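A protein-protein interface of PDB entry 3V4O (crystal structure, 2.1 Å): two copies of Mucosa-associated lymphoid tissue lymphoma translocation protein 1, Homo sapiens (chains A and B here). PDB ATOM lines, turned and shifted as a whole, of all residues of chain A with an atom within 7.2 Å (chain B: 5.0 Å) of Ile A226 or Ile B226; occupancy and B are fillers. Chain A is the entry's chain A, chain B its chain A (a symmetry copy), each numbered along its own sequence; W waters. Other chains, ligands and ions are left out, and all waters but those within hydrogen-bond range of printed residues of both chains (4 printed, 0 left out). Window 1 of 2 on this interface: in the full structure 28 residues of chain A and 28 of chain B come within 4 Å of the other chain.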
ATOM      1  N   ARG A 141     -10.153  -4.274  10.622  1.00  0.00           N
ATOM      2  CA  ARG A 141     -11.106  -5.204  10.036  1.00  0.00           C
ATOM      3  C   ARG A 141     -11.125  -6.533  10.817  1.00  0.00           C
ATOM      4  O   ARG A 141     -11.181  -7.603  10.230  1.00  0.00           O
ATOM      5  CB  ARG A 141     -10.716  -5.459   8.577  1.00  0.00           C
ATOM      6  CG  ARG A 141     -10.893  -4.236   7.627  1.00  0.00           C
ATOM      7  CD  ARG A 141     -10.364  -4.581   6.258  1.00  0.00           C
ATOM      8  NE  ARG A 141     -11.274  -5.497   5.558  1.00  0.00           N
ATOM      9  CZ  ARG A 141     -10.959  -6.128   4.433  1.00  0.00           C
ATOM     10  NH1 ARG A 141      -9.771  -5.922   3.861  1.00  0.00           N
ATOM     11  NH2 ARG A 141     -11.850  -6.926   3.853  1.00  0.00           N
ATOM     12  N   ILE A 162     -17.288  -0.973  -9.023  1.00  0.00           N
ATOM     13  CA  ILE A 162     -17.110  -0.893  -7.594  1.00  0.00           C
ATOM     14  C   ILE A 162     -15.643  -1.107  -7.275  1.00  0.00           C
ATOM     15  O   ILE A 162     -15.056  -2.119  -7.697  1.00  0.00           O
ATOM     16  CB  ILE A 162     -17.925  -2.004  -6.907  1.00  0.00           C
ATOM     17  CG1 ILE A 162     -19.412  -1.799  -7.226  1.00  0.00           C
ATOM     18  CG2 ILE A 162     -17.628  -2.040  -5.388  1.00  0.00           C
ATOM     19  CD1 ILE A 162     -20.292  -3.003  -6.962  1.00  0.00           C
ATOM     20  N   VAL A 163     -15.039  -0.163  -6.550  1.00  0.00           N
ATOM     21  CA  VAL A 163     -13.671  -0.342  -6.088  1.00  0.00           C
ATOM     22  C   VAL A 163     -13.616  -0.109  -4.572  1.00  0.00           C
ATOM     23  O   VAL A 163     -14.051   0.945  -4.099  1.00  0.00           O
ATOM     24  CB  VAL A 163     -12.742   0.652  -6.798  1.00  0.00           C
ATOM     25  CG1 VAL A 163     -11.274   0.403  -6.393  1.00  0.00           C
ATOM     26  CG2 VAL A 163     -12.897   0.536  -8.338  1.00  0.00           C
ATOM     27  N   PHE A 164     -13.085  -1.066  -3.819  1.00  0.00           N
ATOM     28  CA  PHE A 164     -12.758  -0.858  -2.403  1.00  0.00           C
ATOM     29  C   PHE A 164     -11.240  -0.715  -2.291  1.00  0.00           C
ATOM     30  O   PHE A 164     -10.504  -1.537  -2.822  1.00  0.00           O
ATOM     31  CB  PHE A 164     -13.180  -2.059  -1.528  1.00  0.00           C
ATOM     32  CG  PHE A 164     -14.633  -2.083  -1.199  1.00  0.00           C
ATOM     33  CD1 PHE A 164     -15.061  -1.888   0.094  1.00  0.00           C
ATOM     34  CD2 PHE A 164     -15.585  -2.263  -2.201  1.00  0.00           C
ATOM     35  CE1 PHE A 164     -16.423  -1.873   0.405  1.00  0.00           C
ATOM     36  CE2 PHE A 164     -16.936  -2.271  -1.888  1.00  0.00           C
ATOM     37  CZ  PHE A 164     -17.349  -2.044  -0.579  1.00  0.00           C
ATOM     38  N   GLY A 165     -10.784   0.333  -1.617  1.00  0.00           N
ATOM     39  CA  GLY A 165      -9.412   0.391  -1.136  1.00  0.00           C
ATOM     40  C   GLY A 165      -9.429   0.266   0.381  1.00  0.00           C
ATOM     41  O   GLY A 165      -9.721   1.226   1.079  1.00  0.00           O
ATOM     42  N   TYR A 166      -9.158  -0.918   0.904  1.00  0.00           N
ATOM     43  CA  TYR A 166      -9.113  -1.077   2.342  1.00  0.00           C
ATOM     44  C   TYR A 166      -7.670  -0.820   2.797  1.00  0.00           C
ATOM     45  O   TYR A 166      -6.732  -1.428   2.266  1.00  0.00           O
ATOM     46  CB  TYR A 166      -9.441  -2.498   2.767  1.00  0.00           C
ATOM     47  CG  TYR A 166     -10.778  -3.104   2.353  1.00  0.00           C
ATOM     48  CD1 TYR A 166     -11.895  -3.026   3.189  1.00  0.00           C
ATOM     49  CD2 TYR A 166     -10.883  -3.859   1.182  1.00  0.00           C
ATOM     50  CE1 TYR A 166     -13.106  -3.646   2.827  1.00  0.00           C
ATOM     51  CE2 TYR A 166     -12.082  -4.495   0.824  1.00  0.00           C
ATOM     52  CZ  TYR A 166     -13.175  -4.378   1.630  1.00  0.00           C
ATOM     53  OH  TYR A 166     -14.348  -4.999   1.242  1.00  0.00           O
ATOM     54  N   THR A 168      -6.303  -1.983   5.208  1.00  0.00           N
ATOM     55  CA  THR A 168      -5.719  -3.240   5.694  1.00  0.00           C
ATOM     56  C   THR A 168      -6.496  -4.486   5.219  1.00  0.00           C
ATOM     57  O   THR A 168      -7.506  -4.339   4.575  1.00  0.00           O
ATOM     58  CB  THR A 168      -5.548  -3.246   7.234  1.00  0.00           C
ATOM     59  OG1 THR A 168      -4.527  -4.198   7.571  1.00  0.00           O
ATOM     60  CG2 THR A 168      -6.879  -3.621   7.996  1.00  0.00           C
ATOM     61  N   LYS A 200      -6.502   4.703 -13.986  1.00  0.00           N
ATOM     62  CA  LYS A 200      -7.697   4.009 -13.489  1.00  0.00           C
ATOM     63  C   LYS A 200      -7.483   3.809 -11.978  1.00  0.00           C
ATOM     64  O   LYS A 200      -6.383   3.497 -11.562  1.00  0.00           O
ATOM     65  CB  LYS A 200      -7.839   2.657 -14.209  1.00  0.00           C
ATOM     66  CG  LYS A 200      -8.994   1.769 -13.740  1.00  0.00           C
ATOM     67  CD  LYS A 200      -8.938   0.351 -14.431  1.00  0.00           C
ATOM     68  CE  LYS A 200     -10.296  -0.326 -14.244  1.00  0.00           C
ATOM     69  NZ  LYS A 200     -10.406  -1.698 -14.809  1.00  0.00           N
ATOM     70  N   ILE A 201      -8.519   4.031 -11.180  1.00  0.00           N
ATOM     71  CA  ILE A 201      -8.420   4.044  -9.720  1.00  0.00           C
ATOM     72  C   ILE A 201      -7.849   2.700  -9.210  1.00  0.00           C
ATOM     73  O   ILE A 201      -7.067   2.651  -8.255  1.00  0.00           O
ATOM     74  CB  ILE A 201      -9.803   4.446  -9.067  1.00  0.00           C
ATOM     75  CG1 ILE A 201      -9.717   4.476  -7.530  1.00  0.00           C
ATOM     76  CG2 ILE A 201     -10.969   3.548  -9.533  1.00  0.00           C
ATOM     77  CD1 ILE A 201      -8.626   5.419  -7.007  1.00  0.00           C
ATOM     78  N   THR A 202      -8.195   1.612  -9.898  1.00  0.00           N
ATOM     79  CA  THR A 202      -7.697   0.284  -9.532  1.00  0.00           C
ATOM     80  C   THR A 202      -6.183   0.224  -9.605  1.00  0.00           C
ATOM     81  O   THR A 202      -5.522  -0.308  -8.711  1.00  0.00           O
ATOM     82  CB  THR A 202      -8.321  -0.838 -10.407  1.00  0.00           C
ATOM     83  OG1 THR A 202      -9.737  -0.831 -10.230  1.00  0.00           O
ATOM     84  CG2 THR A 202      -7.879  -2.189  -9.871  1.00  0.00           C
ATOM     85  N   VAL A 203      -5.639   0.824 -10.650  1.00  0.00           N
ATOM     86  CA  VAL A 203      -4.223   0.728 -10.917  1.00  0.00           C
ATOM     87  C   VAL A 203      -3.497   1.654  -9.959  1.00  0.00           C
ATOM     88  O   VAL A 203      -2.443   1.330  -9.438  1.00  0.00           O
ATOM     89  CB  VAL A 203      -3.921   1.143 -12.375  1.00  0.00           C
ATOM     90  CG1 VAL A 203      -2.432   1.419 -12.557  1.00  0.00           C
ATOM     91  CG2 VAL A 203      -4.442   0.052 -13.361  1.00  0.00           C
ATOM     92  N   LEU A 204      -4.099   2.814  -9.713  1.00  0.00           N
ATOM     93  CA  LEU A 204      -3.537   3.793  -8.798  1.00  0.00           C
ATOM     94  C   LEU A 204      -3.427   3.176  -7.398  1.00  0.00           C
ATOM     95  O   LEU A 204      -2.421   3.346  -6.708  1.00  0.00           O
ATOM     96  CB  LEU A 204      -4.433   5.035  -8.808  1.00  0.00           C
ATOM     97  CG  LEU A 204      -4.054   6.313  -8.064  1.00  0.00           C
ATOM     98  CD1 LEU A 204      -4.975   7.407  -8.536  1.00  0.00           C
ATOM     99  CD2 LEU A 204      -4.139   6.162  -6.528  1.00  0.00           C
ATOM    100  N   LEU A 205      -4.473   2.460  -6.970  1.00  0.00           N
ATOM    101  CA  LEU A 205      -4.460   1.847  -5.626  1.00  0.00           C
ATOM    102  C   LEU A 205      -3.409   0.742  -5.536  1.00  0.00           C
ATOM    103  O   LEU A 205      -2.817   0.531  -4.481  1.00  0.00           O
ATOM    104  CB  LEU A 205      -5.835   1.265  -5.288  1.00  0.00           C
ATOM    105  CG  LEU A 205      -6.852   1.991  -4.393  1.00  0.00           C
ATOM    106  CD1 LEU A 205      -6.513   3.371  -3.965  1.00  0.00           C
ATOM    107  CD2 LEU A 205      -8.278   1.872  -4.909  1.00  0.00           C
ATOM    108  N   ASP A 206      -3.207   0.023  -6.648  1.00  0.00           N
ATOM    109  CA  ASP A 206      -2.187  -1.006  -6.725  1.00  0.00           C
ATOM    110  C   ASP A 206      -0.765  -0.445  -6.500  1.00  0.00           C
ATOM    111  O   ASP A 206       0.050  -1.081  -5.824  1.00  0.00           O
ATOM    112  CB  ASP A 206      -2.269  -1.736  -8.061  1.00  0.00           C
ATOM    113  CG  ASP A 206      -1.495  -3.064  -8.052  1.00  0.00           C
ATOM    114  OD1 ASP A 206      -1.600  -3.882  -7.084  1.00  0.00           O
ATOM    115  OD2 ASP A 206      -0.767  -3.282  -9.040  1.00  0.00           O
ATOM    116  N   GLU A 207      -0.497   0.744  -7.046  1.00  0.00           N
ATOM    117  CA  GLU A 207       0.777   1.433  -6.834  1.00  0.00           C
ATOM    118  C   GLU A 207       0.927   1.821  -5.376  1.00  0.00           C
ATOM    119  O   GLU A 207       1.984   1.640  -4.814  1.00  0.00           O
ATOM    120  CB  GLU A 207       0.871   2.707  -7.683  1.00  0.00           C
ATOM    121  CG  GLU A 207       1.006   2.459  -9.205  1.00  0.00           C
ATOM    122  CD  GLU A 207       0.795   3.742 -10.005  1.00  0.00           C
ATOM    123  OE1 GLU A 207       0.204   4.717  -9.465  1.00  0.00           O
ATOM    124  OE2 GLU A 207       1.208   3.788 -11.185  1.00  0.00           O
ATOM    125  N   VAL A 208      -0.138   2.363  -4.779  1.00  0.00           N
ATOM    126  CA  VAL A 208      -0.156   2.642  -3.354  1.00  0.00           C
ATOM    127  C   VAL A 208       0.112   1.390  -2.516  1.00  0.00           C
ATOM    128  O   VAL A 208       0.838   1.451  -1.495  1.00  0.00           O
ATOM    129  CB  VAL A 208      -1.484   3.319  -2.917  1.00  0.00           C
ATOM    130  CG1 VAL A 208      -1.494   3.528  -1.388  1.00  0.00           C
ATOM    131  CG2 VAL A 208      -1.669   4.682  -3.634  1.00  0.00           C
ATOM    132  N   ALA A 209      -0.458   0.252  -2.908  1.00  0.00           N
ATOM    133  CA  ALA A 209      -0.162  -1.009  -2.195  1.00  0.00           C
ATOM    134  C   ALA A 209       1.345  -1.340  -2.202  1.00  0.00           C
ATOM    135  O   ALA A 209       1.927  -1.798  -1.203  1.00  0.00           O
ATOM    136  CB  ALA A 209      -0.969  -2.173  -2.787  1.00  0.00           C
ATOM    137  N   ALA A 223      -1.508  -4.293   5.307  1.00  0.00           N
ATOM    138  CA  ALA A 223      -1.283  -4.217   3.865  1.00  0.00           C
ATOM    139  C   ALA A 223      -2.568  -3.789   3.169  1.00  0.00           C
ATOM    140  O   ALA A 223      -3.648  -4.287   3.495  1.00  0.00           O
ATOM    141  CB  ALA A 223      -0.811  -5.580   3.338  1.00  0.00           C
ATOM    142  N   LEU A 224      -2.437  -2.861   2.223  1.00  0.00           N
ATOM    143  CA  LEU A 224      -3.551  -2.402   1.473  1.00  0.00           C
ATOM    144  C   LEU A 224      -4.227  -3.609   0.795  1.00  0.00           C
ATOM    145  O   LEU A 224      -3.539  -4.477   0.266  1.00  0.00           O
ATOM    146  CB  LEU A 224      -3.045  -1.432   0.408  1.00  0.00           C
ATOM    147  CG  LEU A 224      -4.024  -0.354  -0.070  1.00  0.00           C
ATOM    148  CD1 LEU A 224      -3.266   0.755  -0.739  1.00  0.00           C
ATOM    149  CD2 LEU A 224      -5.012  -0.914  -1.052  1.00  0.00           C
ATOM    150  N   GLU A 225      -5.557  -3.676   0.852  1.00  0.00           N
ATOM    151  CA  GLU A 225      -6.314  -4.624   0.038  1.00  0.00           C
ATOM    152  C   GLU A 225      -7.212  -3.907  -0.972  1.00  0.00           C
ATOM    153  O   GLU A 225      -8.022  -3.044  -0.627  1.00  0.00           O
ATOM    154  CB  GLU A 225      -7.129  -5.626   0.884  1.00  0.00           C
ATOM    155  CG  GLU A 225      -7.714  -6.739   0.000  1.00  0.00           C
ATOM    156  CD  GLU A 225      -8.374  -7.857   0.769  1.00  0.00           C
ATOM    157  OE1 GLU A 225      -9.396  -7.592   1.444  1.00  0.00           O
ATOM    158  OE2 GLU A 225      -7.863  -9.006   0.687  1.00  0.00           O
ATOM    159  N   ILE A 226      -7.061  -4.256  -2.233  1.00  0.00           N
ATOM    160  CA  ILE A 226      -7.943  -3.729  -3.248  1.00  0.00           C
ATOM    161  C   ILE A 226      -8.947  -4.797  -3.606  1.00  0.00           C
ATOM    162  O   ILE A 226      -8.583  -5.980  -3.762  1.00  0.00           O
ATOM    163  CB  ILE A 226      -7.177  -3.416  -4.495  1.00  0.00           C
ATOM    164  CG1 ILE A 226      -6.028  -2.477  -4.169  1.00  0.00           C
ATOM    165  CG2 ILE A 226      -8.107  -2.784  -5.544  1.00  0.00           C
ATOM    166  CD1 ILE A 226      -5.008  -2.334  -5.305  1.00  0.00           C
ATOM    167  N   ARG A 227     -10.210  -4.403  -3.722  1.00  0.00           N
ATOM    168  CA  ARG A 227     -11.214  -5.310  -4.210  1.00  0.00           C
ATOM    169  C   ARG A 227     -12.012  -4.541  -5.229  1.00  0.00           C
ATOM    170  O   ARG A 227     -12.598  -3.519  -4.901  1.00  0.00           O
ATOM    171  CB  ARG A 227     -12.108  -5.816  -3.084  1.00  0.00           C
ATOM    172  CG  ARG A 227     -13.160  -6.768  -3.626  1.00  0.00           C
ATOM    173  CD  ARG A 227     -13.851  -7.569  -2.555  1.00  0.00           C
ATOM    174  NE  ARG A 227     -14.581  -6.752  -1.586  1.00  0.00           N
ATOM    175  CZ  ARG A 227     -15.800  -6.254  -1.776  1.00  0.00           C
ATOM    176  NH1 ARG A 227     -16.420  -6.437  -2.931  1.00  0.00           N
ATOM    177  NH2 ARG A 227     -16.383  -5.536  -0.817  1.00  0.00           N
ATOM    178  N   SER A 228     -12.032  -5.022  -6.472  1.00  0.00           N
ATOM    179  CA  SER A 228     -12.558  -4.235  -7.580  1.00  0.00           C
ATOM    180  C   SER A 228     -13.289  -5.111  -8.585  1.00  0.00           C
ATOM    181  O   SER A 228     -12.769  -6.171  -8.988  1.00  0.00           O
ATOM    182  CB  SER A 228     -11.394  -3.549  -8.314  1.00  0.00           C
ATOM    183  OG  SER A 228     -11.782  -2.976  -9.558  1.00  0.00           O
ATOM    184  N   SER A 229     -14.461  -4.652  -9.016  1.00  0.00           N
ATOM    185  CA  SER A 229     -15.094  -5.216 -10.203  1.00  0.00           C
ATOM    186  C   SER A 229     -15.241  -4.146 -11.292  1.00  0.00           C
ATOM    187  O   SER A 229     -15.985  -4.309 -12.257  1.00  0.00           O
ATOM    188  CB  SER A 229     -16.441  -5.857  -9.840  1.00  0.00           C
ATOM    189  OG  SER A 229     -17.364  -4.914  -9.329  1.00  0.00           O
ATOM    190  N   LEU A 230     -14.490  -3.057 -11.159  1.00  0.00           N
ATOM    191  CA  LEU A 230     -14.567  -1.993 -12.144  1.00  0.00           C
ATOM    192  C   LEU A 230     -14.021  -2.482 -13.497  1.00  0.00           C
ATOM    193  O   LEU A 230     -12.842  -2.798 -13.604  1.00  0.00           O
ATOM    194  CB  LEU A 230     -13.777  -0.770 -11.635  1.00  0.00           C
ATOM    195  CG  LEU A 230     -13.614   0.402 -12.618  1.00  0.00           C
ATOM    196  CD1 LEU A 230     -15.000   0.979 -13.009  1.00  0.00           C
ATOM    197  CD2 LEU A 230     -12.724   1.484 -12.011  1.00  0.00           C
ATOM    198  N   VAL B 163      -3.505 -12.845  -4.404  1.00  0.00           N
ATOM    199  CA  VAL B 163      -4.375 -12.310  -5.441  1.00  0.00           C
ATOM    200  C   VAL B 163      -5.505 -13.311  -5.717  1.00  0.00           C
ATOM    201  O   VAL B 163      -5.231 -14.480  -6.005  1.00  0.00           O
ATOM    202  CB  VAL B 163      -3.574 -12.068  -6.727  1.00  0.00           C
ATOM    203  CG1 VAL B 163      -4.462 -11.405  -7.801  1.00  0.00           C
ATOM    204  CG2 VAL B 163      -2.336 -11.178  -6.435  1.00  0.00           C
ATOM    205  N   PHE B 164      -6.756 -12.869  -5.641  1.00  0.00           N
ATOM    206  CA  PHE B 164      -7.897 -13.658  -6.117  1.00  0.00           C
ATOM    207  C   PHE B 164      -8.365 -13.051  -7.440  1.00  0.00           C
ATOM    208  O   PHE B 164      -8.566 -11.846  -7.527  1.00  0.00           O
ATOM    209  CB  PHE B 164      -9.088 -13.608  -5.133  1.00  0.00           C
ATOM    210  CG  PHE B 164      -8.937 -14.515  -3.960  1.00  0.00           C
ATOM    211  CD1 PHE B 164      -9.762 -15.605  -3.808  1.00  0.00           C
ATOM    212  CD2 PHE B 164      -7.932 -14.297  -3.019  1.00  0.00           C
ATOM    213  CE1 PHE B 164      -9.604 -16.480  -2.730  1.00  0.00           C
ATOM    214  CE2 PHE B 164      -7.790 -15.153  -1.936  1.00  0.00           C
ATOM    215  CZ  PHE B 164      -8.617 -16.266  -1.816  1.00  0.00           C
ATOM    216  N   GLY B 165      -8.521 -13.884  -8.461  1.00  0.00           N
ATOM    217  CA  GLY B 165      -9.288 -13.510  -9.639  1.00  0.00           C
ATOM    218  C   GLY B 165     -10.578 -14.319  -9.649  1.00  0.00           C
ATOM    219  O   GLY B 165     -10.576 -15.485 -10.013  1.00  0.00           O
ATOM    220  N   THR B 202      -1.919  -8.597 -10.780  1.00  0.00           N
ATOM    221  CA  THR B 202      -3.031  -7.708 -10.438  1.00  0.00           C
ATOM    222  C   THR B 202      -3.450  -6.866 -11.626  1.00  0.00           C
ATOM    223  O   THR B 202      -4.639  -6.711 -11.913  1.00  0.00           O
ATOM    224  CB  THR B 202      -2.700  -6.796  -9.224  1.00  0.00           C
ATOM    225  OG1 THR B 202      -2.421  -7.616  -8.090  1.00  0.00           O
ATOM    226  CG2 THR B 202      -3.946  -6.020  -8.833  1.00  0.00           C
ATOM    227  N   LEU B 205      -4.971  -8.967 -14.480  1.00  0.00           N
ATOM    228  CA  LEU B 205      -6.374  -9.348 -14.220  1.00  0.00           C
ATOM    229  C   LEU B 205      -7.315  -8.163 -14.438  1.00  0.00           C
ATOM    230  O   LEU B 205      -8.453  -8.342 -14.864  1.00  0.00           O
ATOM    231  CB  LEU B 205      -6.535  -9.863 -12.787  1.00  0.00           C
ATOM    232  CG  LEU B 205      -6.596 -11.358 -12.438  1.00  0.00           C
ATOM    233  CD1 LEU B 205      -6.349 -12.320 -13.543  1.00  0.00           C
ATOM    234  CD2 LEU B 205      -5.814 -11.700 -11.179  1.00  0.00           C
ATOM    235  N   ASP B 206      -6.832  -6.956 -14.115  1.00  0.00           N
ATOM    236  CA  ASP B 206      -7.589  -5.739 -14.341  1.00  0.00           C
ATOM    237  C   ASP B 206      -7.911  -5.513 -15.836  1.00  0.00           C
ATOM    238  O   ASP B 206      -9.021  -5.088 -16.172  1.00  0.00           O
ATOM    239  CB  ASP B 206      -6.848  -4.537 -13.767  1.00  0.00           C
ATOM    240  CG  ASP B 206      -7.752  -3.302 -13.625  1.00  0.00           C
ATOM    241  OD1 ASP B 206      -8.918  -3.393 -13.127  1.00  0.00           O
ATOM    242  OD2 ASP B 206      -7.274  -2.224 -14.027  1.00  0.00           O
ATOM    243  N   ALA B 209     -10.568  -7.890 -16.717  1.00  0.00           N
ATOM    244  CA  ALA B 209     -11.869  -7.347 -16.271  1.00  0.00           C
ATOM    245  C   ALA B 209     -12.476  -6.372 -17.303  1.00  0.00           C
ATOM    246  O   ALA B 209     -13.690  -6.366 -17.573  1.00  0.00           O
ATOM    247  CB  ALA B 209     -11.735  -6.663 -14.903  1.00  0.00           C
ATOM    248  N   LEU B 224     -15.715  -9.867 -13.630  1.00  0.00           N
ATOM    249  CA  LEU B 224     -14.546 -10.286 -12.944  1.00  0.00           C
ATOM    250  C   LEU B 224     -14.402  -9.459 -11.652  1.00  0.00           C
ATOM    251  O   LEU B 224     -14.612  -8.250 -11.674  1.00  0.00           O
ATOM    252  CB  LEU B 224     -13.343 -10.035 -13.849  1.00  0.00           C
ATOM    253  CG  LEU B 224     -12.123 -10.942 -13.650  1.00  0.00           C
ATOM    254  CD1 LEU B 224     -11.246 -10.882 -14.867  1.00  0.00           C
ATOM    255  CD2 LEU B 224     -11.314 -10.510 -12.460  1.00  0.00           C
ATOM    256  N   GLU B 225     -14.089 -10.119 -10.536  1.00  0.00           N
ATOM    257  CA  GLU B 225     -13.681  -9.420  -9.321  1.00  0.00           C
ATOM    258  C   GLU B 225     -12.234  -9.745  -8.942  1.00  0.00           C
ATOM    259  O   GLU B 225     -11.840 -10.906  -8.808  1.00  0.00           O
ATOM    260  CB  GLU B 225     -14.630  -9.679  -8.130  1.00  0.00           C
ATOM    261  CG  GLU B 225     -14.299  -8.747  -6.953  1.00  0.00           C
ATOM    262  CD  GLU B 225     -15.291  -8.809  -5.819  1.00  0.00           C
ATOM    263  OE1 GLU B 225     -15.403  -9.884  -5.185  1.00  0.00           O
ATOM    264  OE2 GLU B 225     -15.953  -7.769  -5.561  1.00  0.00           O
ATOM    265  N   ILE B 226     -11.431  -8.714  -8.783  1.00  0.00           N
ATOM    266  CA  ILE B 226     -10.080  -8.906  -8.308  1.00  0.00           C
ATOM    267  C   ILE B 226     -10.029  -8.520  -6.850  1.00  0.00           C
ATOM    268  O   ILE B 226     -10.605  -7.489  -6.450  1.00  0.00           O
ATOM    269  CB  ILE B 226      -9.137  -7.999  -9.032  1.00  0.00           C
ATOM    270  CG1 ILE B 226      -9.269  -8.212 -10.532  1.00  0.00           C
ATOM    271  CG2 ILE B 226      -7.691  -8.263  -8.577  1.00  0.00           C
ATOM    272  CD1 ILE B 226      -8.576  -7.131 -11.370  1.00  0.00           C
ATOM    273  N   ARG B 227      -9.364  -9.341  -6.046  1.00  0.00           N
ATOM    274  CA  ARG B 227      -9.127  -8.981  -4.673  1.00  0.00           C
ATOM    275  C   ARG B 227      -7.676  -9.284  -4.407  1.00  0.00           C
ATOM    276  O   ARG B 227      -7.254 -10.424  -4.545  1.00  0.00           O
ATOM    277  CB  ARG B 227     -10.030  -9.760  -3.726  1.00  0.00           C
ATOM    278  CG  ARG B 227      -9.757  -9.365  -2.284  1.00  0.00           C
ATOM    279  CD  ARG B 227     -10.826  -9.820  -1.326  1.00  0.00           C
ATOM    280  NE  ARG B 227     -10.986 -11.273  -1.270  1.00  0.00           N
ATOM    281  CZ  ARG B 227     -10.221 -12.095  -0.557  1.00  0.00           C
ATOM    282  NH1 ARG B 227      -9.191 -11.619   0.126  1.00  0.00           N
ATOM    283  NH2 ARG B 227     -10.466 -13.404  -0.560  1.00  0.00           N
ATOM    284  N   SER B 228      -6.903  -8.264  -4.033  1.00  0.00           N
ATOM    285  CA  SER B 228      -5.451  -8.390  -3.992  1.00  0.00           C
ATOM    286  C   SER B 228      -4.860  -7.615  -2.827  1.00  0.00           C
ATOM    287  O   SER B 228      -5.219  -6.440  -2.608  1.00  0.00           O
ATOM    288  CB  SER B 228      -4.854  -7.819  -5.288  1.00  0.00           C
ATOM    289  OG  SER B 228      -3.441  -7.660  -5.227  1.00  0.00           O
HETATM  290  O   HOH W   1     -15.137  -6.522 -13.636  1.00  0.00           O
HETATM  291  O   HOH W   2     -11.021  -4.124 -11.835  1.00  0.00           O
HETATM  292  O   HOH W   3     -17.153  -5.542  -6.535  1.00  0.00           O
HETATM  293  O   HOH W   4      -2.395  -5.220  -5.035  1.00  0.00           O
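Thr A202 touches Asp B206. OD1 of Asp A206 touches CG2 of Thr B202, at 3.6 Å. Leu A224 touches Ser B228. Ser B228 touches Glu A225. Ile B226 touches Ile A226. O of Ile A226 touches CA of Arg B227, at 3.2 Å. O of Ile B226 touches CA of Arg A227 (3.2 Å). CD of Arg A227 touches CD of Arg B227, at 3.97 Å. Ser A228 touches Leu B224 (O to O, 3.9 Å). Ser A228 touches Glu B225.
Of the 25 printed residues of chain A, 11 touch a printed residue of chain B. Of the 12 printed residues of chain B, 7 touch a printed residue of chain A. Printed residues of chain B that touch a printed residue of chain A: Thr B202, Asp B206, Leu B224, Glu B225, Ile B226, Arg B227 and Ser B228. Among the printed residues, 18 pairs touch across the chains. Among the printed residues, Asp or Glu carboxylates within 4 Å of a Lys or Arg side-chain nitrogen of the other chain: Lys A200 with Asp B206, Glu A225 with Arg B227 and Arg A227 with Glu B225.
O of Glu A225 is in hydrogen-bond range of N of Tyr A166 (2.9 Å). NZ of Lys A200 is in hydrogen-bond range of O of Leu A230. The side-chain hydroxyl (OG) of Ser A228 sits at hydrogen-bond distance from the side-chain hydroxyl (OG1) of Thr A202. OE1 of Glu A225 lies within salt-bridge range of NH1 of Arg A141 (3.0 Å). The backbone NH (N) of Phe A164 sits at hydrogen-bond distance from the backbone carbonyl oxygen (O) of Arg A227. The backbone NH (N) of Phe B164 is in hydrogen-bond range of the backbone carbonyl oxygen (O) of Arg B227, 2.7 Å away.
Water W2 lies within hydrogen-bond range of the side-chain carboxylate of Asp B206 (2.6 Å), the side-chain hydroxyl of Ser A228 (2.7 Å) and the backbone carbonyl oxygen of Leu A230 (2.9 Å). Water W4 bridges OD1 of Asp A206 (2.6 Å) and OG of Ser B228 (2.7 Å). Water W1 bridges O of Leu B224 (2.7 Å) and O of Ser A229 (2.7 Å). Water W3 lies within hydrogen-bond range of OE2 of Glu B225 (2.7 Å) and OG of Ser A229 (2.9 Å).
Of chain B, only Ile B226 (3.7 Å), Arg B227 (3.2 Å) and Ser B228 (2.8 Å) come within 4 Å of Ile A226. Printed residues of chain A within 4 Å of Ile B226: Ile A226 (3.7 Å), Arg A227 (3.2 Å) and Ser A228 (2.9 Å). Of the printed residues of chain B, Ser A229 touches Leu B224. Of the printed residues of chain B, Glu A225 touches Arg B227 (3.0 Å) and Ser B228 (3.4 Å). The nearest residue of chain A that does not touch Ile B226 is Ser A229 (5.1 Å).
Thr A202 touches Asp B206, and with the chains exchanged Asp A206 touches Thr B202. Glu A225 touches Arg B227, and with the chains exchanged Arg A227 touches Glu B225. Ile A226 touches Ser B228, and with the chains exchanged Ser A228 touches Ile B226. Arg B227 touches its own counterpart, Arg A227.
NH1 of Arg A227 is in salt-bridge range of OE2 of Glu B225, at 3.0 Å. O of Ile A226 is in hydrogen-bond range of N of Ser B228, at 2.8 Å. NZ of Lys A200 is in salt-bridge range of OD1 of Asp B206, 2.8 Å away. The backbone NH (N) of Ser A228 lies within hydrogen-bond range of the backbone carbonyl oxygen (O) of Ile B226 (2.9 Å). The guanidinium group of Arg B227 is in salt-bridge range of the side-chain carboxylate of Glu A225 (3.0 Å).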
